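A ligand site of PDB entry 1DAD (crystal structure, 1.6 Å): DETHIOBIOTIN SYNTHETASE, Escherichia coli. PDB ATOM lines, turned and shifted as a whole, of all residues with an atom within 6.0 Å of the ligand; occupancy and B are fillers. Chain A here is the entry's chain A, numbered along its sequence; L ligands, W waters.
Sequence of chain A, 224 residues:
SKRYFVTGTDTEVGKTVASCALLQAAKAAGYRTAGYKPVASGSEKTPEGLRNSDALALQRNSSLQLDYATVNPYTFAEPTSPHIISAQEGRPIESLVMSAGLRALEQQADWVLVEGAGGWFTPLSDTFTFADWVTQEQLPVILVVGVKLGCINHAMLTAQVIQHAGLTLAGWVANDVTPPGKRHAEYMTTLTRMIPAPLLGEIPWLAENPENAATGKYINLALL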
ATOM      1  N   ASP A  10      15.113  16.199  15.905  1.00  0.00           N
ATOM      2  CA  ASP A  10      15.152  14.923  15.197  1.00  0.00           C
ATOM      3  C   ASP A  10      15.147  13.797  16.243  1.00  0.00           C
ATOM      4  O   ASP A  10      15.389  14.056  17.421  1.00  0.00           O
ATOM      5  CB  ASP A  10      16.440  14.882  14.366  1.00  0.00           C
ATOM      6  CG  ASP A  10      16.490  13.874  13.213  1.00  0.00           C
ATOM      7  OD1 ASP A  10      15.820  12.845  13.255  1.00  0.00           O
ATOM      8  OD2 ASP A  10      17.195  14.164  12.245  1.00  0.00           O
ATOM      9  N   THR A  11      14.819  12.550  15.864  1.00  0.00           N
ATOM     10  CA  THR A  11      14.933  11.402  16.758  1.00  0.00           C
ATOM     11  C   THR A  11      16.415  11.300  17.159  1.00  0.00           C
ATOM     12  O   THR A  11      17.312  11.797  16.452  1.00  0.00           O
ATOM     13  CB  THR A  11      14.380  10.129  15.973  1.00  0.00           C
ATOM     14  OG1 THR A  11      14.868  10.079  14.626  1.00  0.00           O
ATOM     15  CG2 THR A  11      12.864  10.225  15.901  1.00  0.00           C
ATOM     16  N   GLU A  12      16.686  10.820  18.373  1.00  0.00           N
ATOM     17  CA  GLU A  12      18.042  10.627  18.839  1.00  0.00           C
ATOM     18  C   GLU A  12      18.912  11.900  18.884  1.00  0.00           C
ATOM     19  O   GLU A  12      20.115  11.876  18.607  1.00  0.00           O
ATOM     20  CB  GLU A  12      18.682   9.531  17.966  1.00  0.00           C
ATOM     21  CG  GLU A  12      18.936   8.165  18.610  1.00  0.00           C
ATOM     22  CD  GLU A  12      17.727   7.404  19.151  1.00  0.00           C
ATOM     23  OE1 GLU A  12      16.916   6.900  18.356  1.00  0.00           O
ATOM     24  OE2 GLU A  12      17.624   7.275  20.368  1.00  0.00           O
ATOM     25  N   VAL A  13      18.357  13.055  19.283  1.00  0.00           N
ATOM     26  CA  VAL A  13      19.171  14.272  19.481  1.00  0.00           C
ATOM     27  C   VAL A  13      19.569  14.439  20.941  1.00  0.00           C
ATOM     28  O   VAL A  13      20.210  15.417  21.308  1.00  0.00           O
ATOM     29  CB  VAL A  13      18.468  15.625  19.080  1.00  0.00           C
ATOM     30  CG1 VAL A  13      18.484  15.746  17.584  1.00  0.00           C
ATOM     31  CG2 VAL A  13      17.050  15.694  19.566  1.00  0.00           C
ATOM     32  N   GLY A  14      19.124  13.514  21.809  1.00  0.00           N
ATOM     33  CA  GLY A  14      19.394  13.597  23.239  1.00  0.00           C
ATOM     34  C   GLY A  14      18.278  14.288  23.980  1.00  0.00           C
ATOM     35  O   GLY A  14      18.539  14.931  24.994  1.00  0.00           O
ATOM     36  N   LYS A  15      17.027  14.206  23.523  1.00  0.00           N
ATOM     37  CA  LYS A  15      15.904  14.790  24.226  1.00  0.00           C
ATOM     38  C   LYS A  15      15.775  14.218  25.662  1.00  0.00           C
ATOM     39  O   LYS A  15      15.518  14.965  26.609  1.00  0.00           O
ATOM     40  CB  LYS A  15      14.710  14.522  23.370  1.00  0.00           C
ATOM     41  CG  LYS A  15      13.369  14.985  23.835  1.00  0.00           C
ATOM     42  CD  LYS A  15      12.296  14.707  22.760  1.00  0.00           C
ATOM     43  CE  LYS A  15      12.160  13.248  22.269  1.00  0.00           C
ATOM     44  NZ  LYS A  15      12.829  13.140  20.979  1.00  0.00           N
ATOM     45  N   THR A  16      16.061  12.935  25.913  1.00  0.00           N
ATOM     46  CA  THR A  16      15.989  12.440  27.279  1.00  0.00           C
ATOM     47  C   THR A  16      17.167  12.930  28.125  1.00  0.00           C
ATOM     48  O   THR A  16      16.991  13.272  29.302  1.00  0.00           O
ATOM     49  CB  THR A  16      15.906  10.902  27.252  1.00  0.00           C
ATOM     50  OG1 THR A  16      14.742  10.572  26.469  1.00  0.00           O
ATOM     51  CG2 THR A  16      15.752  10.260  28.645  1.00  0.00           C
ATOM     52  N   VAL A  17      18.375  13.056  27.554  1.00  0.00           N
ATOM     53  CA  VAL A  17      19.539  13.537  28.281  1.00  0.00           C
ATOM     54  C   VAL A  17      19.321  14.985  28.752  1.00  0.00           C
ATOM     55  O   VAL A  17      19.574  15.324  29.922  1.00  0.00           O
ATOM     56  CB  VAL A  17      20.802  13.438  27.376  1.00  0.00           C
ATOM     57  CG1 VAL A  17      22.004  14.166  27.939  1.00  0.00           C
ATOM     58  CG2 VAL A  17      21.166  11.950  27.265  1.00  0.00           C
ATOM     59  N   ALA A  18      18.802  15.806  27.857  1.00  0.00           N
ATOM     60  CA  ALA A  18      18.461  17.166  28.190  1.00  0.00           C
ATOM     61  C   ALA A  18      17.300  17.192  29.213  1.00  0.00           C
ATOM     62  O   ALA A  18      17.359  18.033  30.111  1.00  0.00           O
ATOM     63  CB  ALA A  18      18.057  17.890  26.940  1.00  0.00           C
ATOM     64  N   LYS A  37       6.195  11.004  30.698  1.00  0.00           N
ATOM     65  CA  LYS A  37       6.343  10.591  29.320  1.00  0.00           C
ATOM     66  C   LYS A  37       5.075   9.799  28.948  1.00  0.00           C
ATOM     67  O   LYS A  37       4.973   8.600  29.201  1.00  0.00           O
ATOM     68  CB  LYS A  37       7.662   9.738  29.158  1.00  0.00           C
ATOM     69  CG  LYS A  37       7.849   9.437  27.655  1.00  0.00           C
ATOM     70  CD  LYS A  37       9.266   9.123  27.256  1.00  0.00           C
ATOM     71  CE  LYS A  37       9.354   8.673  25.783  1.00  0.00           C
ATOM     72  NZ  LYS A  37       9.974   9.704  24.979  1.00  0.00           N
ATOM     73  N   ASP A  54      13.703   5.503  28.483  1.00  0.00           N
ATOM     74  CA  ASP A  54      13.594   6.951  28.661  1.00  0.00           C
ATOM     75  C   ASP A  54      12.671   7.317  29.809  1.00  0.00           C
ATOM     76  O   ASP A  54      13.024   8.148  30.650  1.00  0.00           O
ATOM     77  CB  ASP A  54      13.082   7.624  27.381  1.00  0.00           C
ATOM     78  CG  ASP A  54      14.097   7.446  26.241  1.00  0.00           C
ATOM     79  OD1 ASP A  54      15.312   7.361  26.450  1.00  0.00           O
ATOM     80  OD2 ASP A  54      13.708   7.424  25.100  1.00  0.00           O
ATOM     81  N   GLU A 115       7.704  14.918  28.300  1.00  0.00           N
ATOM     82  CA  GLU A 115       8.577  14.592  27.216  1.00  0.00           C
ATOM     83  C   GLU A 115       7.706  13.980  26.151  1.00  0.00           C
ATOM     84  O   GLU A 115       6.887  13.106  26.448  1.00  0.00           O
ATOM     85  CB  GLU A 115       9.654  13.610  27.693  1.00  0.00           C
ATOM     86  CG  GLU A 115      10.790  13.523  26.727  1.00  0.00           C
ATOM     87  CD  GLU A 115      11.872  12.540  27.146  1.00  0.00           C
ATOM     88  OE1 GLU A 115      12.693  12.863  28.001  1.00  0.00           O
ATOM     89  OE2 GLU A 115      11.904  11.438  26.618  1.00  0.00           O
ATOM     90  N   ASN A 175      22.664  20.295  22.613  1.00  0.00           N
ATOM     91  CA  ASN A 175      23.187  19.050  23.063  1.00  0.00           C
ATOM     92  C   ASN A 175      24.318  18.555  22.149  1.00  0.00           C
ATOM     93  O   ASN A 175      24.132  18.404  20.938  1.00  0.00           O
ATOM     94  CB  ASN A 175      22.065  18.044  23.133  1.00  0.00           C
ATOM     95  CG  ASN A 175      22.536  16.752  23.814  1.00  0.00           C
ATOM     96  OD1 ASN A 175      23.480  16.712  24.577  1.00  0.00           O
ATOM     97  ND2 ASN A 175      21.952  15.602  23.559  1.00  0.00           N
ATOM     98  N   ASP A 176      25.537  18.357  22.637  1.00  0.00           N
ATOM     99  CA  ASP A 176      26.635  17.922  21.816  1.00  0.00           C
ATOM    100  C   ASP A 176      26.655  16.421  21.714  1.00  0.00           C
ATOM    101  O   ASP A 176      27.189  15.693  22.548  1.00  0.00           O
ATOM    102  CB  ASP A 176      27.948  18.409  22.383  1.00  0.00           C
ATOM    103  CG  ASP A 176      28.041  19.926  22.550  1.00  0.00           C
ATOM    104  OD1 ASP A 176      27.287  20.652  21.927  1.00  0.00           O
ATOM    105  OD2 ASP A 176      28.879  20.398  23.297  1.00  0.00           O
ATOM    106  N   VAL A 177      25.990  15.983  20.662  1.00  0.00           N
ATOM    107  CA  VAL A 177      25.912  14.555  20.383  1.00  0.00           C
ATOM    108  C   VAL A 177      27.190  13.963  19.781  1.00  0.00           C
ATOM    109  O   VAL A 177      27.391  12.737  19.843  1.00  0.00           O
ATOM    110  CB  VAL A 177      24.665  14.287  19.475  1.00  0.00           C
ATOM    111  CG1 VAL A 177      23.448  14.542  20.362  1.00  0.00           C
ATOM    112  CG2 VAL A 177      24.649  15.150  18.197  1.00  0.00           C
ATOM    113  N   ILE A 203      24.925  21.024  26.742  1.00  0.00           N
ATOM    114  CA  ILE A 203      25.402  19.818  27.378  1.00  0.00           C
ATOM    115  C   ILE A 203      26.560  19.299  26.516  1.00  0.00           C
ATOM    116  O   ILE A 203      26.375  19.064  25.306  1.00  0.00           O
ATOM    117  CB  ILE A 203      24.275  18.809  27.457  1.00  0.00           C
ATOM    118  CG1 ILE A 203      23.181  19.445  28.306  1.00  0.00           C
ATOM    119  CG2 ILE A 203      24.714  17.480  28.068  1.00  0.00           C
ATOM    120  CD1 ILE A 203      21.853  18.742  28.026  1.00  0.00           C
ATOM    121  N   PRO A 204      27.754  19.095  27.073  1.00  0.00           N
ATOM    122  CA  PRO A 204      28.897  18.558  26.353  1.00  0.00           C
ATOM    123  C   PRO A 204      28.750  17.094  25.950  1.00  0.00           C
ATOM    124  O   PRO A 204      27.886  16.377  26.484  1.00  0.00           O
ATOM    125  CB  PRO A 204      30.068  18.809  27.286  1.00  0.00           C
ATOM    126  CG  PRO A 204      29.434  18.647  28.635  1.00  0.00           C
ATOM    127  CD  PRO A 204      28.102  19.376  28.460  1.00  0.00           C
ATOM    128  N   TRP A 205      29.654  16.648  25.072  1.00  0.00           N
ATOM    129  CA  TRP A 205      29.684  15.270  24.629  1.00  0.00           C
ATOM    130  C   TRP A 205      30.093  14.421  25.829  1.00  0.00           C
ATOM    131  O   TRP A 205      31.141  14.651  26.425  1.00  0.00           O
ATOM    132  CB  TRP A 205      30.688  15.163  23.441  1.00  0.00           C
ATOM    133  CG  TRP A 205      30.805  13.739  22.940  1.00  0.00           C
ATOM    134  CD1 TRP A 205      29.691  13.075  22.450  1.00  0.00           C
ATOM    135  CD2 TRP A 205      31.939  12.938  23.054  1.00  0.00           C
ATOM    136  NE1 TRP A 205      30.100  11.852  22.295  1.00  0.00           N
ATOM    137  CE2 TRP A 205      31.411  11.703  22.636  1.00  0.00           C
ATOM    138  CE3 TRP A 205      33.282  13.035  23.456  1.00  0.00           C
ATOM    139  CZ2 TRP A 205      32.234  10.558  22.598  1.00  0.00           C
ATOM    140  CZ3 TRP A 205      34.074  11.902  23.419  1.00  0.00           C
ATOM    141  CH2 TRP A 205      33.551  10.672  23.006  1.00  0.00           C
ATOM    142  N   LEU A 206      29.300  13.489  26.307  1.00  0.00           N
ATOM    143  CA  LEU A 206      29.645  12.686  27.469  1.00  0.00           C
ATOM    144  C   LEU A 206      29.501  11.212  27.076  1.00  0.00           C
ATOM    145  O   LEU A 206      28.442  10.590  26.970  1.00  0.00           O
ATOM    146  CB  LEU A 206      28.716  13.034  28.642  1.00  0.00           C
ATOM    147  CG  LEU A 206      28.799  14.448  29.219  1.00  0.00           C
ATOM    148  CD1 LEU A 206      27.503  14.760  29.872  1.00  0.00           C
ATOM    149  CD2 LEU A 206      29.925  14.588  30.191  1.00  0.00           C
ATOM    150  N   ALA A 207      30.666  10.623  26.839  1.00  0.00           N
ATOM    151  CA  ALA A 207      30.810   9.243  26.370  1.00  0.00           C
ATOM    152  C   ALA A 207      30.135   8.070  27.132  1.00  0.00           C
ATOM    153  O   ALA A 207      29.782   7.048  26.535  1.00  0.00           O
ATOM    154  CB  ALA A 207      32.299   9.008  26.260  1.00  0.00           C
ATOM    155  N   ASN A 209      27.173   6.710  29.676  1.00  0.00           N
ATOM    156  CA  ASN A 209      25.812   6.811  30.229  1.00  0.00           C
ATOM    157  C   ASN A 209      25.239   8.199  30.610  1.00  0.00           C
ATOM    158  O   ASN A 209      24.736   8.372  31.749  1.00  0.00           O
ATOM    159  CB  ASN A 209      25.719   5.867  31.476  1.00  0.00           C
ATOM    160  CG  ASN A 209      26.015   4.385  31.212  1.00  0.00           C
ATOM    161  OD1 ASN A 209      26.968   4.043  30.512  1.00  0.00           O
ATOM    162  ND2 ASN A 209      25.201   3.462  31.720  1.00  0.00           N
ATOM    163  N   PRO A 210      25.183   9.205  29.686  1.00  0.00           N
ATOM    164  CA  PRO A 210      24.952  10.615  30.013  1.00  0.00           C
ATOM    165  C   PRO A 210      23.631  10.881  30.743  1.00  0.00           C
ATOM    166  O   PRO A 210      23.437  11.955  31.307  1.00  0.00           O
ATOM    167  CB  PRO A 210      25.089  11.313  28.647  1.00  0.00           C
ATOM    168  CG  PRO A 210      24.605  10.285  27.653  1.00  0.00           C
ATOM    169  CD  PRO A 210      25.245   9.023  28.217  1.00  0.00           C
ATOM    170  N   GLU A 211      22.696   9.913  30.758  1.00  0.00           N
ATOM    171  CA  GLU A 211      21.418   9.997  31.479  1.00  0.00           C
ATOM    172  C   GLU A 211      21.637   9.954  33.010  1.00  0.00           C
ATOM    173  O   GLU A 211      20.874  10.517  33.795  1.00  0.00           O
ATOM    174  CB  GLU A 211      20.485   8.837  31.161  1.00  0.00           C
ATOM    175  CG  GLU A 211      20.377   8.489  29.689  1.00  0.00           C
ATOM    176  CD  GLU A 211      21.523   7.667  29.040  1.00  0.00           C
ATOM    177  OE1 GLU A 211      22.235   6.964  29.772  1.00  0.00           O
ATOM    178  OE2 GLU A 211      21.692   7.734  27.806  1.00  0.00           O
HETATM  179  P1  LIG L   1      16.156  11.081  22.358  1.00  0.00           P
HETATM  180  O1  LIG L   1      16.002  12.211  21.399  1.00  0.00           O
HETATM  181  O2  LIG L   1      15.265  11.242  23.712  1.00  0.00           O
HETATM  182  O3  LIG L   1      15.832   9.775  21.714  1.00  0.00           O
HETATM  183  P2  LIG L   1      18.354  10.379  24.057  1.00  0.00           P
HETATM  184  O4  LIG L   1      17.579   9.175  24.415  1.00  0.00           O
HETATM  185  O5  LIG L   1      18.518  11.288  25.206  1.00  0.00           O
HETATM  186  O6  LIG L   1      17.619  11.109  22.889  1.00  0.00           O
HETATM  187  O7  LIG L   1      19.768  10.014  23.393  1.00  0.00           O
HETATM  188  C1  LIG L   1      19.842   9.168  22.237  1.00  0.00           C
HETATM  189  C2  LIG L   1      21.252   8.583  22.213  1.00  0.00           C
HETATM  190  O8  LIG L   1      22.204   9.656  22.083  1.00  0.00           O
HETATM  191  C3  LIG L   1      21.603   7.852  23.506  1.00  0.00           C
HETATM  192  O9  LIG L   1      22.482   6.759  23.265  1.00  0.00           O
HETATM  193  C4  LIG L   1      22.355   8.902  24.310  1.00  0.00           C
HETATM  194  O10 LIG L   1      23.190   8.313  25.312  1.00  0.00           O
HETATM  195  C5  LIG L   1      23.099   9.625  23.210  1.00  0.00           C
HETATM  196  N1  LIG L   1      23.474  11.017  23.616  1.00  0.00           N
HETATM  197  C6  LIG L   1      22.596  12.007  23.789  1.00  0.00           C
HETATM  198  N2  LIG L   1      23.234  13.063  24.308  1.00  0.00           N
HETATM  199  C7  LIG L   1      24.492  12.750  24.467  1.00  0.00           C
HETATM  200  C8  LIG L   1      25.604  13.412  24.943  1.00  0.00           C
HETATM  201  N3  LIG L   1      25.497  14.648  25.441  1.00  0.00           N
HETATM  202  N4  LIG L   1      26.812  12.786  24.953  1.00  0.00           N
HETATM  203  C9  LIG L   1      26.937  11.529  24.515  1.00  0.00           C
HETATM  204  N5  LIG L   1      25.867  10.884  24.068  1.00  0.00           N
HETATM  205  C10 LIG L   1      24.651  11.442  24.013  1.00  0.00           C
HETATM  206  O   HOH W   1      18.839   8.717  26.780  1.00  0.00           O
HETATM  207  O   HOH W   2      16.273   7.033  23.891  1.00  0.00           O
HETATM  208  O   HOH W   3      13.014  10.057  23.950  1.00  0.00           O
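The side-chain carboxylate (OE2) of Glu 211 is in hydrogen-bond range of an oxygen (O10) of the ligand (3.0 Å). N of Val 17 sits at hydrogen-bond distance from O5 of the ligand (2.9 Å). N4 of the ligand sits at hydrogen-bond distance from N of Leu 206, 2.9 Å away. The side-chain hydroxyl (OG1) of Thr 16 is in hydrogen-bond range of an oxygen (O2) of the ligand (2.9 Å). The side-chain amino group (NZ) of Lys 15 is in salt-bridge range of an oxygen (O1) of the ligand, at 3.3 Å. The backbone NH (N) of Gly 14 is in hydrogen-bond range of an oxygen (O6) of the ligand (3.0 Å). N of Lys 15 is in hydrogen-bond range of O1 of the ligand, 3.1 Å away. N of Val 13 sits at hydrogen-bond distance from O1 of the ligand. O1 of the ligand sits at hydrogen-bond distance from N of Glu 12. The side-chain amide nitrogen (ND2) of Asn 175 lies within hydrogen-bond range of a nitrogen (N2) of the ligand (2.9 Å). A nitrogen (N3) of the ligand lies within hydrogen-bond range of the backbone carbonyl oxygen of Pro 204, at 3.1 Å. The backbone NH (N) of Thr 16 is in hydrogen-bond range of an oxygen (O2) of the ligand.
The side-chain hydroxyl (OG1) of Thr 16 lies within hydrogen-bond range of the side-chain carboxylate (OE2) of Glu 115 (3.0 Å). The backbone carbonyl oxygen of Val 13 lies within hydrogen-bond range of the side-chain amide nitrogen of Asn 175 (2.9 Å). OD1 of Asp 54 lies close to OG1 of Thr 16 (3.3 Å). The backbone NH (N) of Asp 176 lies within hydrogen-bond range of the backbone carbonyl oxygen (O) of Ile 203, at 2.9 Å.
Merely in contact with the ligand: Asp 54 (3.5 Å), Asp 176 (3.5 Å), Ile 203 (3.9 Å), Trp 205 (3.8 Å) and Pro 210 (3.4 Å). Hydrophobic or aromatic side chains that line the ligand: Val 17, Ile 203, Trp 205 and Pro 210. 15 residues have an atom within 4 Å of the ligand: Glu 12, Val 13, Gly 14, Lys 15, Thr 16, Val 17, Asp 54, Asn 175, Asp 176, Ile 203, Pro 204, Trp 205, Leu 206, Pro 210 and Glu 211. The nearest printed residue that does not touch the ligand is Val 177 (4.2 Å).
Water W3 lies within hydrogen-bond range of O2 of the ligand (2.6 Å), OD2 of Asp 54 (3.0 Å), OG1 of Thr 16 (3.1 Å), OE2 of Glu 115 (3.2 Å) and NZ of Lys 37 (3.2 Å). Water W2 lies within hydrogen-bond range of O4 of the ligand (2.6 Å) and OD1 of Asp 54 (2.8 Å). Water W1 bridges O4 of the ligand and OE2 of Glu 211.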
